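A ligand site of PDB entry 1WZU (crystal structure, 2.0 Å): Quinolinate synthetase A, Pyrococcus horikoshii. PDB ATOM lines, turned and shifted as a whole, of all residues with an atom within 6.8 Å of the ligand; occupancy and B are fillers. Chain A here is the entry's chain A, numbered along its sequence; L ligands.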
ATOM      1  N   HIS A  21     -13.616 -12.141   5.192  1.00  0.00           N
ATOM      2  CA  HIS A  21     -13.624 -10.706   5.557  1.00  0.00           C
ATOM      3  C   HIS A  21     -14.403  -9.957   4.481  1.00  0.00           C
ATOM      4  O   HIS A  21     -14.470 -10.400   3.333  1.00  0.00           O
ATOM      5  CB  HIS A  21     -12.206 -10.181   5.722  1.00  0.00           C
ATOM      6  CG  HIS A  21     -12.109  -8.717   6.049  1.00  0.00           C
ATOM      7  ND1 HIS A  21     -11.869  -7.802   5.018  1.00  0.00           N
ATOM      8  CD2 HIS A  21     -12.303  -7.994   7.152  1.00  0.00           C
ATOM      9  CE1 HIS A  21     -11.824  -6.603   5.534  1.00  0.00           C
ATOM     10  NE2 HIS A  21     -12.121  -6.668   6.814  1.00  0.00           N
ATOM     11  N   ASN A  22     -14.864  -8.759   4.830  1.00  0.00           N
ATOM     12  CA  ASN A  22     -15.541  -7.917   3.879  1.00  0.00           C
ATOM     13  C   ASN A  22     -14.751  -7.540   2.653  1.00  0.00           C
ATOM     14  O   ASN A  22     -15.322  -7.148   1.636  1.00  0.00           O
ATOM     15  CB  ASN A  22     -16.219  -6.753   4.556  1.00  0.00           C
ATOM     16  CG  ASN A  22     -17.365  -7.138   5.491  1.00  0.00           C
ATOM     17  OD1 ASN A  22     -18.324  -7.807   5.070  1.00  0.00           O
ATOM     18  ND2 ASN A  22     -17.309  -6.670   6.717  1.00  0.00           N
ATOM     19  N   TYR A  23     -13.448  -7.556   2.657  1.00  0.00           N
ATOM     20  CA  TYR A  23     -12.675  -7.136   1.476  1.00  0.00           C
ATOM     21  C   TYR A  23     -12.402  -8.272   0.515  1.00  0.00           C
ATOM     22  O   TYR A  23     -11.787  -8.058  -0.525  1.00  0.00           O
ATOM     23  CB  TYR A  23     -11.324  -6.529   1.872  1.00  0.00           C
ATOM     24  CG  TYR A  23     -11.384  -5.275   2.700  1.00  0.00           C
ATOM     25  CD1 TYR A  23     -12.451  -4.386   2.601  1.00  0.00           C
ATOM     26  CD2 TYR A  23     -10.325  -4.947   3.563  1.00  0.00           C
ATOM     27  CE1 TYR A  23     -12.491  -3.216   3.357  1.00  0.00           C
ATOM     28  CE2 TYR A  23     -10.351  -3.780   4.317  1.00  0.00           C
ATOM     29  CZ  TYR A  23     -11.431  -2.917   4.212  1.00  0.00           C
ATOM     30  OH  TYR A  23     -11.463  -1.783   4.987  1.00  0.00           O
ATOM     31  N   GLY A  36     -17.853 -10.808   7.394  1.00  0.00           N
ATOM     32  CA  GLY A  36     -17.969  -9.670   8.307  1.00  0.00           C
ATOM     33  C   GLY A  36     -16.655  -8.935   8.495  1.00  0.00           C
ATOM     34  O   GLY A  36     -15.687  -9.192   7.776  1.00  0.00           O
ATOM     35  N   ASP A  37     -16.626  -8.008   9.453  1.00  0.00           N
ATOM     36  CA  ASP A  37     -15.405  -7.259   9.734  1.00  0.00           C
ATOM     37  C   ASP A  37     -14.607  -8.024  10.808  1.00  0.00           C
ATOM     38  O   ASP A  37     -15.021  -9.110  11.219  1.00  0.00           O
ATOM     39  CB  ASP A  37     -15.733  -5.821  10.185  1.00  0.00           C
ATOM     40  CG  ASP A  37     -16.433  -5.757  11.518  1.00  0.00           C
ATOM     41  OD1 ASP A  37     -16.653  -6.818  12.142  1.00  0.00           O
ATOM     42  OD2 ASP A  37     -16.758  -4.630  11.966  1.00  0.00           O
ATOM     43  N   SER A  38     -13.480  -7.493  11.267  1.00  0.00           N
ATOM     44  CA  SER A  38     -12.680  -8.218  12.251  1.00  0.00           C
ATOM     45  C   SER A  38     -13.363  -8.592  13.553  1.00  0.00           C
ATOM     46  O   SER A  38     -13.166  -9.705  14.058  1.00  0.00           O
ATOM     47  CB  SER A  38     -11.385  -7.470  12.551  1.00  0.00           C
ATOM     48  OG  SER A  38     -10.536  -7.514  11.409  1.00  0.00           O
ATOM     49  N   LEU A  39     -14.141  -7.685  14.108  1.00  0.00           N
ATOM     50  CA  LEU A  39     -14.843  -7.962  15.350  1.00  0.00           C
ATOM     51  C   LEU A  39     -15.884  -9.063  15.129  1.00  0.00           C
ATOM     52  O   LEU A  39     -15.956 -10.026  15.898  1.00  0.00           O
ATOM     53  CB  LEU A  39     -15.547  -6.701  15.868  1.00  0.00           C
ATOM     54  CG  LEU A  39     -16.415  -6.911  17.111  1.00  0.00           C
ATOM     55  CD1 LEU A  39     -15.578  -7.485  18.257  1.00  0.00           C
ATOM     56  CD2 LEU A  39     -17.040  -5.583  17.509  1.00  0.00           C
ATOM     57  N   GLU A  40     -16.674  -8.930  14.071  1.00  0.00           N
ATOM     58  CA  GLU A  40     -17.698  -9.927  13.754  1.00  0.00           C
ATOM     59  C   GLU A  40     -17.058 -11.295  13.509  1.00  0.00           C
ATOM     60  O   GLU A  40     -17.601 -12.310  13.920  1.00  0.00           O
ATOM     61  CB  GLU A  40     -18.507  -9.463  12.534  1.00  0.00           C
ATOM     62  CG  GLU A  40     -19.405  -8.264  12.836  1.00  0.00           C
ATOM     63  CD  GLU A  40     -19.806  -7.492  11.598  1.00  0.00           C
ATOM     64  OE1 GLU A  40     -19.368  -7.862  10.483  1.00  0.00           O
ATOM     65  OE2 GLU A  40     -20.567  -6.509  11.741  1.00  0.00           O
ATOM     66  N   PHE A  60      -2.955 -11.584  10.146  1.00  0.00           N
ATOM     67  CA  PHE A  60      -3.112 -11.283  11.559  1.00  0.00           C
ATOM     68  C   PHE A  60      -4.488 -11.643  12.119  1.00  0.00           C
ATOM     69  O   PHE A  60      -4.609 -11.905  13.322  1.00  0.00           O
ATOM     70  CB  PHE A  60      -2.770  -9.821  11.857  1.00  0.00           C
ATOM     71  CG  PHE A  60      -3.590  -8.826  11.093  1.00  0.00           C
ATOM     72  CD1 PHE A  60      -4.949  -8.654  11.367  1.00  0.00           C
ATOM     73  CD2 PHE A  60      -2.999  -8.043  10.103  1.00  0.00           C
ATOM     74  CE1 PHE A  60      -5.699  -7.725  10.670  1.00  0.00           C
ATOM     75  CE2 PHE A  60      -3.756  -7.108   9.396  1.00  0.00           C
ATOM     76  CZ  PHE A  60      -5.110  -6.951   9.685  1.00  0.00           C
ATOM     77  N   MET A  61      -5.519 -11.653  11.282  1.00  0.00           N
ATOM     78  CA  MET A  61      -6.843 -12.021  11.787  1.00  0.00           C
ATOM     79  C   MET A  61      -7.013 -13.527  11.796  1.00  0.00           C
ATOM     80  O   MET A  61      -7.773 -14.061  12.601  1.00  0.00           O
ATOM     81  CB  MET A  61      -7.959 -11.366  10.963  1.00  0.00           C
ATOM     82  CG  MET A  61      -8.483 -10.093  11.630  1.00  0.00           C
ATOM     83  SD  MET A  61      -8.924 -10.360  13.370  1.00  0.00           S
ATOM     84  CE  MET A  61     -10.469 -11.298  13.211  1.00  0.00           C
ATOM     85  N   TYR A 109      -4.252  -2.649  17.998  1.00  0.00           N
ATOM     86  CA  TYR A 109      -5.207  -2.862  16.907  1.00  0.00           C
ATOM     87  C   TYR A 109      -4.982  -4.311  16.467  1.00  0.00           C
ATOM     88  O   TYR A 109      -3.852  -4.785  16.487  1.00  0.00           O
ATOM     89  CB  TYR A 109      -4.877  -1.873  15.791  1.00  0.00           C
ATOM     90  CG  TYR A 109      -5.810  -1.854  14.603  1.00  0.00           C
ATOM     91  CD1 TYR A 109      -7.158  -2.215  14.727  1.00  0.00           C
ATOM     92  CD2 TYR A 109      -5.366  -1.398  13.366  1.00  0.00           C
ATOM     93  CE1 TYR A 109      -8.035  -2.106  13.642  1.00  0.00           C
ATOM     94  CE2 TYR A 109      -6.229  -1.293  12.281  1.00  0.00           C
ATOM     95  CZ  TYR A 109      -7.553  -1.647  12.421  1.00  0.00           C
ATOM     96  OH  TYR A 109      -8.403  -1.516  11.343  1.00  0.00           O
ATOM     97  N   VAL A 110      -6.047  -5.009  16.084  1.00  0.00           N
ATOM     98  CA  VAL A 110      -5.896  -6.400  15.658  1.00  0.00           C
ATOM     99  C   VAL A 110      -4.949  -6.514  14.470  1.00  0.00           C
ATOM    100  O   VAL A 110      -4.395  -7.581  14.225  1.00  0.00           O
ATOM    101  CB  VAL A 110      -7.260  -7.055  15.317  1.00  0.00           C
ATOM    102  CG1 VAL A 110      -8.022  -7.326  16.608  1.00  0.00           C
ATOM    103  CG2 VAL A 110      -8.063  -6.165  14.387  1.00  0.00           C
ATOM    104  N   ASN A 111      -4.781  -5.420  13.730  1.00  0.00           N
ATOM    105  CA  ASN A 111      -3.874  -5.393  12.585  1.00  0.00           C
ATOM    106  C   ASN A 111      -2.457  -5.335  13.170  1.00  0.00           C
ATOM    107  O   ASN A 111      -1.799  -4.303  13.108  1.00  0.00           O
ATOM    108  CB  ASN A 111      -4.116  -4.147  11.722  1.00  0.00           C
ATOM    109  CG  ASN A 111      -5.459  -4.163  11.015  1.00  0.00           C
ATOM    110  OD1 ASN A 111      -6.497  -4.481  11.609  1.00  0.00           O
ATOM    111  ND2 ASN A 111      -5.464  -3.792   9.742  1.00  0.00           N
ATOM    112  N   VAL A 124      -8.152  -4.134  19.957  1.00  0.00           N
ATOM    113  CA  VAL A 124      -9.320  -3.433  19.407  1.00  0.00           C
ATOM    114  C   VAL A 124      -9.364  -3.594  17.893  1.00  0.00           C
ATOM    115  O   VAL A 124      -8.356  -3.892  17.255  1.00  0.00           O
ATOM    116  CB  VAL A 124      -9.320  -1.908  19.709  1.00  0.00           C
ATOM    117  CG1 VAL A 124      -9.351  -1.658  21.211  1.00  0.00           C
ATOM    118  CG2 VAL A 124      -8.091  -1.235  19.072  1.00  0.00           C
ATOM    119  N   THR A 125     -10.567  -3.418  17.347  1.00  0.00           N
ATOM    120  CA  THR A 125     -10.782  -3.454  15.910  1.00  0.00           C
ATOM    121  C   THR A 125     -11.294  -2.058  15.600  1.00  0.00           C
ATOM    122  O   THR A 125     -11.474  -1.246  16.524  1.00  0.00           O
ATOM    123  CB  THR A 125     -11.878  -4.486  15.495  1.00  0.00           C
ATOM    124  OG1 THR A 125     -13.165  -3.991  15.890  1.00  0.00           O
ATOM    125  CG2 THR A 125     -11.627  -5.829  16.164  1.00  0.00           C
ATOM    126  N   SER A 126     -11.531  -1.752  14.327  1.00  0.00           N
ATOM    127  CA  SER A 126     -12.022  -0.431  13.940  1.00  0.00           C
ATOM    128  C   SER A 126     -13.406  -0.131  14.492  1.00  0.00           C
ATOM    129  O   SER A 126     -13.735   1.026  14.774  1.00  0.00           O
ATOM    130  CB  SER A 126     -12.050  -0.289  12.422  1.00  0.00           C
ATOM    131  OG  SER A 126     -10.752  -0.319  11.879  1.00  0.00           O
ATOM    132  N   ALA A 127     -14.218  -1.168  14.654  1.00  0.00           N
ATOM    133  CA  ALA A 127     -15.584  -1.007  15.159  1.00  0.00           C
ATOM    134  C   ALA A 127     -15.696  -0.722  16.656  1.00  0.00           C
ATOM    135  O   ALA A 127     -16.613  -0.010  17.086  1.00  0.00           O
ATOM    136  CB  ALA A 127     -16.395  -2.247  14.816  1.00  0.00           C
ATOM    137  N   LEU A 149      -5.949   5.511  13.088  1.00  0.00           N
ATOM    138  CA  LEU A 149      -7.003   5.034  13.959  1.00  0.00           C
ATOM    139  C   LEU A 149      -6.775   5.646  15.334  1.00  0.00           C
ATOM    140  O   LEU A 149      -7.720   5.940  16.061  1.00  0.00           O
ATOM    141  CB  LEU A 149      -6.979   3.500  14.038  1.00  0.00           C
ATOM    142  CG  LEU A 149      -7.946   2.795  15.007  1.00  0.00           C
ATOM    143  CD1 LEU A 149      -9.379   3.174  14.686  1.00  0.00           C
ATOM    144  CD2 LEU A 149      -7.749   1.282  14.899  1.00  0.00           C
ATOM    145  N   HIS A 196     -13.345   5.081   6.232  1.00  0.00           N
ATOM    146  CA  HIS A 196     -12.792   4.159   7.212  1.00  0.00           C
ATOM    147  C   HIS A 196     -11.875   4.933   8.159  1.00  0.00           C
ATOM    148  O   HIS A 196     -11.175   5.844   7.720  1.00  0.00           O
ATOM    149  CB  HIS A 196     -12.018   3.053   6.483  1.00  0.00           C
ATOM    150  CG  HIS A 196     -11.738   1.850   7.331  1.00  0.00           C
ATOM    151  ND1 HIS A 196     -10.718   1.818   8.252  1.00  0.00           N
ATOM    152  CD2 HIS A 196     -12.379   0.657   7.425  1.00  0.00           C
ATOM    153  CE1 HIS A 196     -10.734   0.655   8.886  1.00  0.00           C
ATOM    154  NE2 HIS A 196     -11.731  -0.063   8.394  1.00  0.00           N
ATOM    155  N   PRO A 197     -11.877   4.587   9.453  1.00  0.00           N
ATOM    156  CA  PRO A 197     -11.021   5.280  10.426  1.00  0.00           C
ATOM    157  C   PRO A 197      -9.520   5.159  10.161  1.00  0.00           C
ATOM    158  O   PRO A 197      -8.696   5.798  10.824  1.00  0.00           O
ATOM    159  CB  PRO A 197     -11.434   4.667  11.764  1.00  0.00           C
ATOM    160  CG  PRO A 197     -11.902   3.287  11.369  1.00  0.00           C
ATOM    161  CD  PRO A 197     -12.713   3.581  10.123  1.00  0.00           C
ATOM    162  N   GLU A 198      -9.168   4.316   9.197  1.00  0.00           N
ATOM    163  CA  GLU A 198      -7.782   4.141   8.812  1.00  0.00           C
ATOM    164  C   GLU A 198      -7.326   5.230   7.837  1.00  0.00           C
ATOM    165  O   GLU A 198      -6.154   5.318   7.508  1.00  0.00           O
ATOM    166  CB  GLU A 198      -7.569   2.759   8.187  1.00  0.00           C
ATOM    167  CG  GLU A 198      -7.230   1.678   9.193  1.00  0.00           C
ATOM    168  CD  GLU A 198      -6.874   0.367   8.531  1.00  0.00           C
ATOM    169  OE1 GLU A 198      -6.227   0.410   7.453  1.00  0.00           O
ATOM    170  OE2 GLU A 198      -7.224  -0.697   9.074  1.00  0.00           O
ATOM    171  N   ALA A 211     -16.570   4.558   9.996  1.00  0.00           N
ATOM    172  CA  ALA A 211     -16.866   3.241  10.550  1.00  0.00           C
ATOM    173  C   ALA A 211     -16.061   2.111   9.928  1.00  0.00           C
ATOM    174  O   ALA A 211     -15.431   2.265   8.871  1.00  0.00           O
ATOM    175  CB  ALA A 211     -18.351   2.941  10.384  1.00  0.00           C
ATOM    176  N   SER A 212     -16.070   0.970  10.598  1.00  0.00           N
ATOM    177  CA  SER A 212     -15.383  -0.199  10.071  1.00  0.00           C
ATOM    178  C   SER A 212     -16.323  -0.666   8.959  1.00  0.00           C
ATOM    179  O   SER A 212     -17.417  -0.115   8.805  1.00  0.00           O
ATOM    180  CB  SER A 212     -15.257  -1.279  11.152  1.00  0.00           C
ATOM    181  OG  SER A 212     -16.516  -1.853  11.456  1.00  0.00           O
ATOM    182  N   THR A 213     -15.906  -1.664   8.188  1.00  0.00           N
ATOM    183  CA  THR A 213     -16.770  -2.164   7.121  1.00  0.00           C
ATOM    184  C   THR A 213     -18.069  -2.684   7.733  1.00  0.00           C
ATOM    185  O   THR A 213     -19.135  -2.593   7.127  1.00  0.00           O
ATOM    186  CB  THR A 213     -16.084  -3.294   6.348  1.00  0.00           C
ATOM    187  OG1 THR A 213     -15.748  -4.359   7.263  1.00  0.00           O
ATOM    188  CG2 THR A 213     -14.799  -2.788   5.689  1.00  0.00           C
ATOM    189  N   GLY A 214     -17.986  -3.240   8.941  1.00  0.00           N
ATOM    190  CA  GLY A 214     -19.175  -3.738   9.602  1.00  0.00           C
ATOM    191  C   GLY A 214     -20.120  -2.583   9.897  1.00  0.00           C
ATOM    192  O   GLY A 214     -21.344  -2.730   9.766  1.00  0.00           O
ATOM    193  N   GLY A 215     -19.560  -1.440  10.279  1.00  0.00           N
ATOM    194  CA  GLY A 215     -20.372  -0.272  10.574  1.00  0.00           C
ATOM    195  C   GLY A 215     -20.992   0.328   9.321  1.00  0.00           C
ATOM    196  O   GLY A 215     -22.133   0.808   9.348  1.00  0.00           O
ATOM    197  N   MET A 216     -20.232   0.295   8.230  1.00  0.00           N
ATOM    198  CA  MET A 216     -20.705   0.817   6.952  1.00  0.00           C
ATOM    199  C   MET A 216     -21.938   0.037   6.501  1.00  0.00           C
ATOM    200  O   MET A 216     -22.916   0.619   6.024  1.00  0.00           O
ATOM    201  CB  MET A 216     -19.603   0.681   5.888  1.00  0.00           C
ATOM    202  CG  MET A 216     -18.418   1.610   6.122  1.00  0.00           C
ATOM    203  SD  MET A 216     -17.133   1.331   4.898  1.00  0.00           S
ATOM    204  CE  MET A 216     -15.908   2.570   5.359  1.00  0.00           C
ATOM    205  N   THR A 230     -12.730   2.973   1.076  1.00  0.00           N
ATOM    206  CA  THR A 230     -12.092   1.780   1.617  1.00  0.00           C
ATOM    207  C   THR A 230     -11.787   0.901   0.408  1.00  0.00           C
ATOM    208  O   THR A 230     -11.954   1.349  -0.729  1.00  0.00           O
ATOM    209  CB  THR A 230     -12.989   1.019   2.613  1.00  0.00           C
ATOM    210  OG1 THR A 230     -12.214   0.039   3.310  1.00  0.00           O
ATOM    211  CG2 THR A 230     -14.131   0.310   1.879  1.00  0.00           C
HETATM  212  C1  LIG L   1     -12.641  -3.436   8.683  1.00  0.00           C
HETATM  213  O1  LIG L   1     -13.299  -2.319   8.844  1.00  0.00           O
HETATM  214  O2  LIG L   1     -13.350  -4.461   8.296  1.00  0.00           O
HETATM  215  C2  LIG L   1     -11.163  -3.613   8.902  1.00  0.00           C
HETATM  216  O3  LIG L   1     -10.524  -2.418   9.313  1.00  0.00           O
HETATM  217  C3  LIG L   1     -10.890  -4.655   9.990  1.00  0.00           C
HETATM  218  C4  LIG L   1     -11.468  -4.271  11.339  1.00  0.00           C
HETATM  219  O4  LIG L   1     -10.794  -3.589  12.222  1.00  0.00           O
HETATM  220  O5  LIG L   1     -12.671  -4.590  11.650  1.00  0.00           O
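The backbone NH (N) of Thr 213 is in hydrogen-bond range of an oxygen (O1) of the ligand, 2.8 Å away.
The side-chain hydroxyl (OG1) of Thr 213 sits at hydrogen-bond distance from an oxygen (O2) of the ligand.
NE2 of His 196 is in hydrogen-bond range of O1 of the ligand (2.8 Å).
An oxygen (O4) of the ligand is in hydrogen-bond range of the backbone NH of Ser 126 (2.9 Å).
OG of Ser 126 sits at hydrogen-bond distance from O4 of the ligand (3.3 Å).
O2 of the ligand is in hydrogen-bond range of NE2 of His 21 (2.9 Å).
N of Ser 38 lies within hydrogen-bond range of O5 of the ligand.
O3 of the ligand is in hydrogen-bond range of OH of Tyr 109, at 3.1 Å.
ND1 of His 196 lies close to N of Glu 198 (3.1 Å).
OG of Ser 126 sits at hydrogen-bond distance from OH of Tyr 109, 2.7 Å away.
A ring nitrogen (ND1) of His 21 lies within hydrogen-bond range of the backbone NH of Tyr 23 (2.9 Å).
OH of Tyr 109 sits at hydrogen-bond distance from OE2 of Glu 198, 2.7 Å away.
The side-chain hydroxyl (OG) of Ser 212 sits at hydrogen-bond distance from the side-chain carboxylate (OD2) of Asp 37, at 2.8 Å.
The side-chain hydroxyl of Ser 212 lies close to the backbone NH of Gly 214.
ND2 of Asn 22 lies close to N of Asp 37 (3.1 Å).
OD1 of Asp 37 is in hydrogen-bond range of N of Glu 40, at 2.9 Å.
Merely in contact with the ligand: Asp 37 (3.3 Å), Thr 125 (3.6 Å), Glu 198 (3.7 Å) and Ser 212 (3.2 Å).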
